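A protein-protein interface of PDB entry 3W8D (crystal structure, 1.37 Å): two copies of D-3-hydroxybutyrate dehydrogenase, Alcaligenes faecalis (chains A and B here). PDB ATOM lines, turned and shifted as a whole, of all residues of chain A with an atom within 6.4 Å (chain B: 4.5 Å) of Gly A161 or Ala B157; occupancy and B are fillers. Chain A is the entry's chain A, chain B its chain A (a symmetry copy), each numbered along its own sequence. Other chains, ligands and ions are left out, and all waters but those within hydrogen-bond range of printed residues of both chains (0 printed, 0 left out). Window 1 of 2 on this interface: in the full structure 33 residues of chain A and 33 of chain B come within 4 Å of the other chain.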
ATOM      1  N   LEU A 115      22.630 -27.273  21.565  1.00  0.00           N
ATOM      2  CA  LEU A 115      23.600 -26.202  21.857  1.00  0.00           C
ATOM      3  C   LEU A 115      23.418 -25.753  23.298  1.00  0.00           C
ATOM      4  O   LEU A 115      24.356 -25.803  24.099  1.00  0.00           O
ATOM      5  CB  LEU A 115      23.477 -25.047  20.869  1.00  0.00           C
ATOM      6  CG  LEU A 115      24.436 -23.880  21.099  1.00  0.00           C
ATOM      7  CD1 LEU A 115      25.947 -24.295  21.245  1.00  0.00           C
ATOM      8  CD2 LEU A 115      24.220 -22.814  20.023  1.00  0.00           C
ATOM      9  N   GLY A 145      29.482 -29.995  12.719  1.00  0.00           N
ATOM     10  CA  GLY A 145      30.059 -28.849  13.415  1.00  0.00           C
ATOM     11  C   GLY A 145      31.193 -28.235  12.658  1.00  0.00           C
ATOM     12  O   GLY A 145      31.701 -27.174  13.114  1.00  0.00           O
ATOM     13  N   VAL A 156      23.226 -28.048  11.917  1.00  0.00           N
ATOM     14  CA  VAL A 156      24.584 -27.548  11.537  1.00  0.00           C
ATOM     15  C   VAL A 156      24.913 -26.318  12.342  1.00  0.00           C
ATOM     16  O   VAL A 156      26.030 -26.181  12.891  1.00  0.00           O
ATOM     17  CB  VAL A 156      24.659 -27.263  10.047  1.00  0.00           C
ATOM     18  CG1 VAL A 156      26.015 -26.584   9.686  1.00  0.00           C
ATOM     19  CG2 VAL A 156      24.546 -28.552   9.279  1.00  0.00           C
ATOM     20  N   ALA A 157      23.951 -25.363  12.480  1.00  0.00           N
ATOM     21  CA  ALA A 157      24.210 -24.191  13.328  1.00  0.00           C
ATOM     22  C   ALA A 157      24.497 -24.586  14.757  1.00  0.00           C
ATOM     23  O   ALA A 157      25.473 -24.115  15.354  1.00  0.00           O
ATOM     24  CB  ALA A 157      22.986 -23.274  13.315  1.00  0.00           C
ATOM     25  N   ALA A 158      23.686 -25.495  15.309  1.00  0.00           N
ATOM     26  CA  ALA A 158      23.930 -25.885  16.721  1.00  0.00           C
ATOM     27  C   ALA A 158      25.295 -26.554  16.930  1.00  0.00           C
ATOM     28  O   ALA A 158      25.974 -26.268  17.908  1.00  0.00           O
ATOM     29  CB  ALA A 158      22.809 -26.823  17.208  1.00  0.00           C
ATOM     30  N   LYS A 159      25.617 -27.467  15.959  1.00  0.00           N
ATOM     31  CA  LYS A 159      26.863 -28.213  16.121  1.00  0.00           C
ATOM     32  C   LYS A 159      28.085 -27.332  15.901  1.00  0.00           C
ATOM     33  O   LYS A 159      29.106 -27.511  16.589  1.00  0.00           O
ATOM     34  CB  LYS A 159      26.867 -29.451  15.163  1.00  0.00           C
ATOM     35  CG  LYS A 159      25.847 -30.521  15.570  1.00  0.00           C
ATOM     36  CD  LYS A 159      26.050 -31.052  17.012  1.00  0.00           C
ATOM     37  CE  LYS A 159      25.229 -32.389  17.236  1.00  0.00           C
ATOM     38  NZ  LYS A 159      25.419 -32.925  18.538  1.00  0.00           N
ATOM     39  N   HIS A 160      28.036 -26.390  14.923  1.00  0.00           N
ATOM     40  CA  HIS A 160      29.096 -25.392  14.812  1.00  0.00           C
ATOM     41  C   HIS A 160      29.186 -24.660  16.169  1.00  0.00           C
ATOM     42  O   HIS A 160      30.293 -24.394  16.661  1.00  0.00           O
ATOM     43  CB  HIS A 160      28.800 -24.436  13.654  1.00  0.00           C
ATOM     44  CG  HIS A 160      29.283 -24.912  12.323  1.00  0.00           C
ATOM     45  ND1 HIS A 160      28.786 -26.028  11.684  1.00  0.00           N
ATOM     46  CD2 HIS A 160      30.242 -24.400  11.484  1.00  0.00           C
ATOM     47  CE1 HIS A 160      29.397 -26.223  10.513  1.00  0.00           C
ATOM     48  NE2 HIS A 160      30.286 -25.247  10.357  1.00  0.00           N
ATOM     49  N   GLY A 161      28.034 -24.285  16.720  1.00  0.00           N
ATOM     50  CA  GLY A 161      28.059 -23.598  18.031  1.00  0.00           C
ATOM     51  C   GLY A 161      28.730 -24.398  19.132  1.00  0.00           C
ATOM     52  O   GLY A 161      29.468 -23.878  19.931  1.00  0.00           O
ATOM     53  N   VAL A 162      28.510 -25.743  19.111  1.00  0.00           N
ATOM     54  CA  VAL A 162      29.140 -26.567  20.128  1.00  0.00           C
ATOM     55  C   VAL A 162      30.672 -26.574  19.929  1.00  0.00           C
ATOM     56  O   VAL A 162      31.405 -26.565  20.887  1.00  0.00           O
ATOM     57  CB  VAL A 162      28.602 -28.031  20.051  1.00  0.00           C
ATOM     58  CG1 VAL A 162      29.503 -28.963  20.889  1.00  0.00           C
ATOM     59  CG2 VAL A 162      27.137 -28.109  20.474  1.00  0.00           C
ATOM     60  N   VAL A 163      31.118 -26.651  18.678  1.00  0.00           N
ATOM     61  CA  VAL A 163      32.588 -26.552  18.409  1.00  0.00           C
ATOM     62  C   VAL A 163      33.139 -25.214  18.965  1.00  0.00           C
ATOM     63  O   VAL A 163      34.176 -25.220  19.663  1.00  0.00           O
ATOM     64  CB  VAL A 163      32.835 -26.761  16.959  1.00  0.00           C
ATOM     65  CG1 VAL A 163      34.244 -26.435  16.624  1.00  0.00           C
ATOM     66  CG2 VAL A 163      32.502 -28.232  16.560  1.00  0.00           C
ATOM     67  N   GLY A 164      32.448 -24.089  18.728  1.00  0.00           N
ATOM     68  CA  GLY A 164      32.904 -22.795  19.287  1.00  0.00           C
ATOM     69  C   GLY A 164      32.909 -22.827  20.802  1.00  0.00           C
ATOM     70  O   GLY A 164      33.862 -22.340  21.426  1.00  0.00           O
ATOM     71  N   LEU A 165      31.807 -23.335  21.355  1.00  0.00           N
ATOM     72  CA  LEU A 165      31.708 -23.372  22.810  1.00  0.00           C
ATOM     73  C   LEU A 165      32.772 -24.242  23.477  1.00  0.00           C
ATOM     74  O   LEU A 165      33.322 -23.888  24.541  1.00  0.00           O
ATOM     75  CB  LEU A 165      30.304 -23.891  23.177  1.00  0.00           C
ATOM     76  CG  LEU A 165      30.023 -24.088  24.617  1.00  0.00           C
ATOM     77  CD1 LEU A 165      30.139 -22.816  25.502  1.00  0.00           C
ATOM     78  CD2 LEU A 165      28.646 -24.709  24.818  1.00  0.00           C
ATOM     79  N   THR A 166      33.121 -25.348  22.816  1.00  0.00           N
ATOM     80  CA  THR A 166      34.177 -26.281  23.282  1.00  0.00           C
ATOM     81  C   THR A 166      35.478 -25.436  23.370  1.00  0.00           C
ATOM     82  O   THR A 166      36.214 -25.556  24.358  1.00  0.00           O
ATOM     83  CB  THR A 166      34.342 -27.335  22.188  1.00  0.00           C
ATOM     84  OG1 THR A 166      33.147 -28.172  22.250  1.00  0.00           O
ATOM     85  CG2 THR A 166      35.559 -28.265  22.538  1.00  0.00           C
ATOM     86  N   VAL A 168      35.950 -22.166  23.698  1.00  0.00           N
ATOM     87  CA  VAL A 168      35.891 -21.208  24.852  1.00  0.00           C
ATOM     88  C   VAL A 168      36.128 -21.907  26.164  1.00  0.00           C
ATOM     89  O   VAL A 168      36.914 -21.405  27.024  1.00  0.00           O
ATOM     90  CB  VAL A 168      34.568 -20.427  24.827  1.00  0.00           C
ATOM     91  CG1 VAL A 168      34.520 -19.524  26.052  1.00  0.00           C
ATOM     92  CG2 VAL A 168      34.430 -19.558  23.588  1.00  0.00           C
ATOM     93  N   TRP B 107      23.032 -15.326  27.743  1.00  0.00           N
ATOM     94  CA  TRP B 107      23.160 -16.433  26.729  1.00  0.00           C
ATOM     95  C   TRP B 107      21.956 -16.427  25.870  1.00  0.00           C
ATOM     96  O   TRP B 107      22.059 -16.431  24.637  1.00  0.00           O
ATOM     97  CB  TRP B 107      23.326 -17.766  27.533  1.00  0.00           C
ATOM     98  CG  TRP B 107      23.173 -18.978  26.581  1.00  0.00           C
ATOM     99  CD1 TRP B 107      21.986 -19.583  26.216  1.00  0.00           C
ATOM    100  CD2 TRP B 107      24.224 -19.679  25.839  1.00  0.00           C
ATOM    101  NE1 TRP B 107      22.219 -20.623  25.271  1.00  0.00           N
ATOM    102  CE2 TRP B 107      23.585 -20.664  25.037  1.00  0.00           C
ATOM    103  CE3 TRP B 107      25.643 -19.539  25.816  1.00  0.00           C
ATOM    104  CZ2 TRP B 107      24.303 -21.540  24.177  1.00  0.00           C
ATOM    105  CZ3 TRP B 107      26.317 -20.435  24.955  1.00  0.00           C
ATOM    106  CH2 TRP B 107      25.641 -21.361  24.153  1.00  0.00           C
ATOM    107  N   SER B 153      31.664 -17.100  25.627  1.00  0.00           N
ATOM    108  CA  SER B 153      30.990 -18.365  25.248  1.00  0.00           C
ATOM    109  C   SER B 153      29.786 -18.179  24.378  1.00  0.00           C
ATOM    110  O   SER B 153      29.689 -18.798  23.312  1.00  0.00           O
ATOM    111  CB  SER B 153      30.616 -19.259  26.477  1.00  0.00           C
ATOM    112  OG  SER B 153      29.815 -18.424  27.385  1.00  0.00           O
ATOM    113  N   ALA B 154      28.801 -17.350  24.782  1.00  0.00           N
ATOM    114  CA  ALA B 154      27.581 -17.237  23.966  1.00  0.00           C
ATOM    115  C   ALA B 154      27.863 -16.663  22.602  1.00  0.00           C
ATOM    116  O   ALA B 154      27.273 -17.083  21.591  1.00  0.00           O
ATOM    117  CB  ALA B 154      26.542 -16.298  24.701  1.00  0.00           C
ATOM    118  N   TYR B 155      28.729 -15.632  22.586  1.00  0.00           N
ATOM    119  CA  TYR B 155      28.965 -14.976  21.337  1.00  0.00           C
ATOM    120  C   TYR B 155      29.750 -15.897  20.329  1.00  0.00           C
ATOM    121  O   TYR B 155      29.370 -15.945  19.146  1.00  0.00           O
ATOM    122  CB  TYR B 155      29.788 -13.716  21.654  1.00  0.00           C
ATOM    123  CG  TYR B 155      30.077 -12.822  20.434  1.00  0.00           C
ATOM    124  CD1 TYR B 155      31.241 -12.974  19.680  1.00  0.00           C
ATOM    125  CD2 TYR B 155      29.181 -11.803  20.088  1.00  0.00           C
ATOM    126  CE1 TYR B 155      31.452 -12.103  18.565  1.00  0.00           C
ATOM    127  CE2 TYR B 155      29.401 -10.908  19.079  1.00  0.00           C
ATOM    128  CZ  TYR B 155      30.539 -11.069  18.334  1.00  0.00           C
ATOM    129  OH  TYR B 155      30.742 -10.245  17.264  1.00  0.00           O
ATOM    130  N   VAL B 156      30.788 -16.539  20.833  1.00  0.00           N
ATOM    131  CA  VAL B 156      31.569 -17.489  19.980  1.00  0.00           C
ATOM    132  C   VAL B 156      30.667 -18.599  19.505  1.00  0.00           C
ATOM    133  O   VAL B 156      30.671 -18.971  18.309  1.00  0.00           O
ATOM    134  CB  VAL B 156      32.764 -18.041  20.737  1.00  0.00           C
ATOM    135  CG1 VAL B 156      33.473 -19.154  19.906  1.00  0.00           C
ATOM    136  CG2 VAL B 156      33.749 -16.936  21.001  1.00  0.00           C
ATOM    137  N   ALA B 157      29.826 -19.174  20.408  1.00  0.00           N
ATOM    138  CA  ALA B 157      28.874 -20.201  19.959  1.00  0.00           C
ATOM    139  C   ALA B 157      27.927 -19.668  18.911  1.00  0.00           C
ATOM    140  O   ALA B 157      27.725 -20.301  17.868  1.00  0.00           O
ATOM    141  CB  ALA B 157      28.051 -20.688  21.152  1.00  0.00           C
ATOM    142  N   ALA B 158      27.375 -18.472  19.145  1.00  0.00           N
ATOM    143  CA  ALA B 158      26.421 -17.933  18.143  1.00  0.00           C
ATOM    144  C   ALA B 158      27.069 -17.687  16.773  1.00  0.00           C
ATOM    145  O   ALA B 158      26.469 -17.989  15.750  1.00  0.00           O
ATOM    146  CB  ALA B 158      25.793 -16.627  18.665  1.00  0.00           C
ATOM    147  N   LYS B 159      28.306 -17.102  16.844  1.00  0.00           N
ATOM    148  CA  LYS B 159      28.962 -16.756  15.585  1.00  0.00           C
ATOM    149  C   LYS B 159      29.430 -17.992  14.830  1.00  0.00           C
ATOM    150  O   LYS B 159      29.370 -18.014  13.588  1.00  0.00           O
ATOM    151  CB  LYS B 159      30.144 -15.767  15.858  1.00  0.00           C
ATOM    152  CG  LYS B 159      29.668 -14.382  16.314  1.00  0.00           C
ATOM    153  CD  LYS B 159      28.714 -13.693  15.306  1.00  0.00           C
ATOM    154  CE  LYS B 159      28.563 -12.152  15.643  1.00  0.00           C
ATOM    155  NZ  LYS B 159      27.722 -11.479  14.716  1.00  0.00           N
ATOM    156  N   HIS B 160      29.940 -19.030  15.542  1.00  0.00           N
ATOM    157  CA  HIS B 160      30.208 -20.307  14.886  1.00  0.00           C
ATOM    158  C   HIS B 160      28.888 -20.781  14.240  1.00  0.00           C
ATOM    159  O   HIS B 160      28.895 -21.281  13.105  1.00  0.00           O
ATOM    160  CB  HIS B 160      30.753 -21.316  15.901  1.00  0.00           C
ATOM    161  CG  HIS B 160      32.232 -21.252  16.101  1.00  0.00           C
ATOM    162  ND1 HIS B 160      32.883 -20.169  16.651  1.00  0.00           N
ATOM    163  CD2 HIS B 160      33.212 -22.172  15.821  1.00  0.00           C
ATOM    164  CE1 HIS B 160      34.200 -20.379  16.709  1.00  0.00           C
ATOM    165  NE2 HIS B 160      34.435 -21.591  16.217  1.00  0.00           N
ATOM    166  N   GLY B 161      27.791 -20.684  14.986  1.00  0.00           N
ATOM    167  CA  GLY B 161      26.493 -21.103  14.408  1.00  0.00           C
ATOM    168  C   GLY B 161      26.119 -20.365  13.137  1.00  0.00           C
ATOM    169  O   GLY B 161      25.625 -20.936  12.197  1.00  0.00           O
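Of the printed residues of chain B, Gly A161 touches Ala B157.
Printed residues of chain A within 4 Å of Ala B157: Gly A161 (3.3 Å).
Printed residues of chain B within 4 Å of Leu A115: Trp B107.
Of the printed residues of chain A, His B160 touches His A160 and Gly A164.
Printed residues of chain A within 4 Å of Val B156: Gly A164 (3.6 Å) and Val A168 (3.6 Å).
Printed residues of chain B within 4 Å of Gly A164: Val B156 and His B160.
The nearest printed residue of chain B that does not touch Gly A164 is Ala B157 (4.8 Å).
Among the printed residues, merely in contact across the chains: His A160 with His B160, Ala A157 with Gly B161, Gly A161 with Ala B157, Gly A164 with His B160, Gly A164 with Val B156, Val A168 with Val B156, Leu A165 with Ser B153, Val A168 with Ser B153 and Leu A115 with Trp B107.
A ring nitrogen (ND1) of His A160 sits close to the backbone carbonyl oxygen of Gly A145 (3.4 Å).
The backbone carbonyl oxygen (O) of Val A156 lies within hydrogen-bond range of a ring nitrogen (ND1) of His A160 (3.0 Å).
O of Val B156 lies within hydrogen-bond range of ND1 of His B160 (3.0 Å).
Printed residues of chain B that touch a printed residue of chain A: Trp B107, Ser B153, Val B156, Ala B157, His B160 and Gly B161.
Hydrophobic or aromatic side chains of chain A within 4 Å of the printed part of chain B: Leu A115, Ala A157, His A160, Leu A165 and Val A168.
Among the printed residues, 9 pairs touch across the chains.
Among the printed residues, no Asp or Glu carboxylate lies within 4 Å of a Lys or Arg side-chain nitrogen of the other chain.
Ala A157 touches Gly B161, and with the chains exchanged Gly A161 touches Ala B157.
His A160 touches its own counterpart, His B160.
Of the 9 pairs that touch across the chains among the printed residues, 3 have their exchanged pair printed and touching as well.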
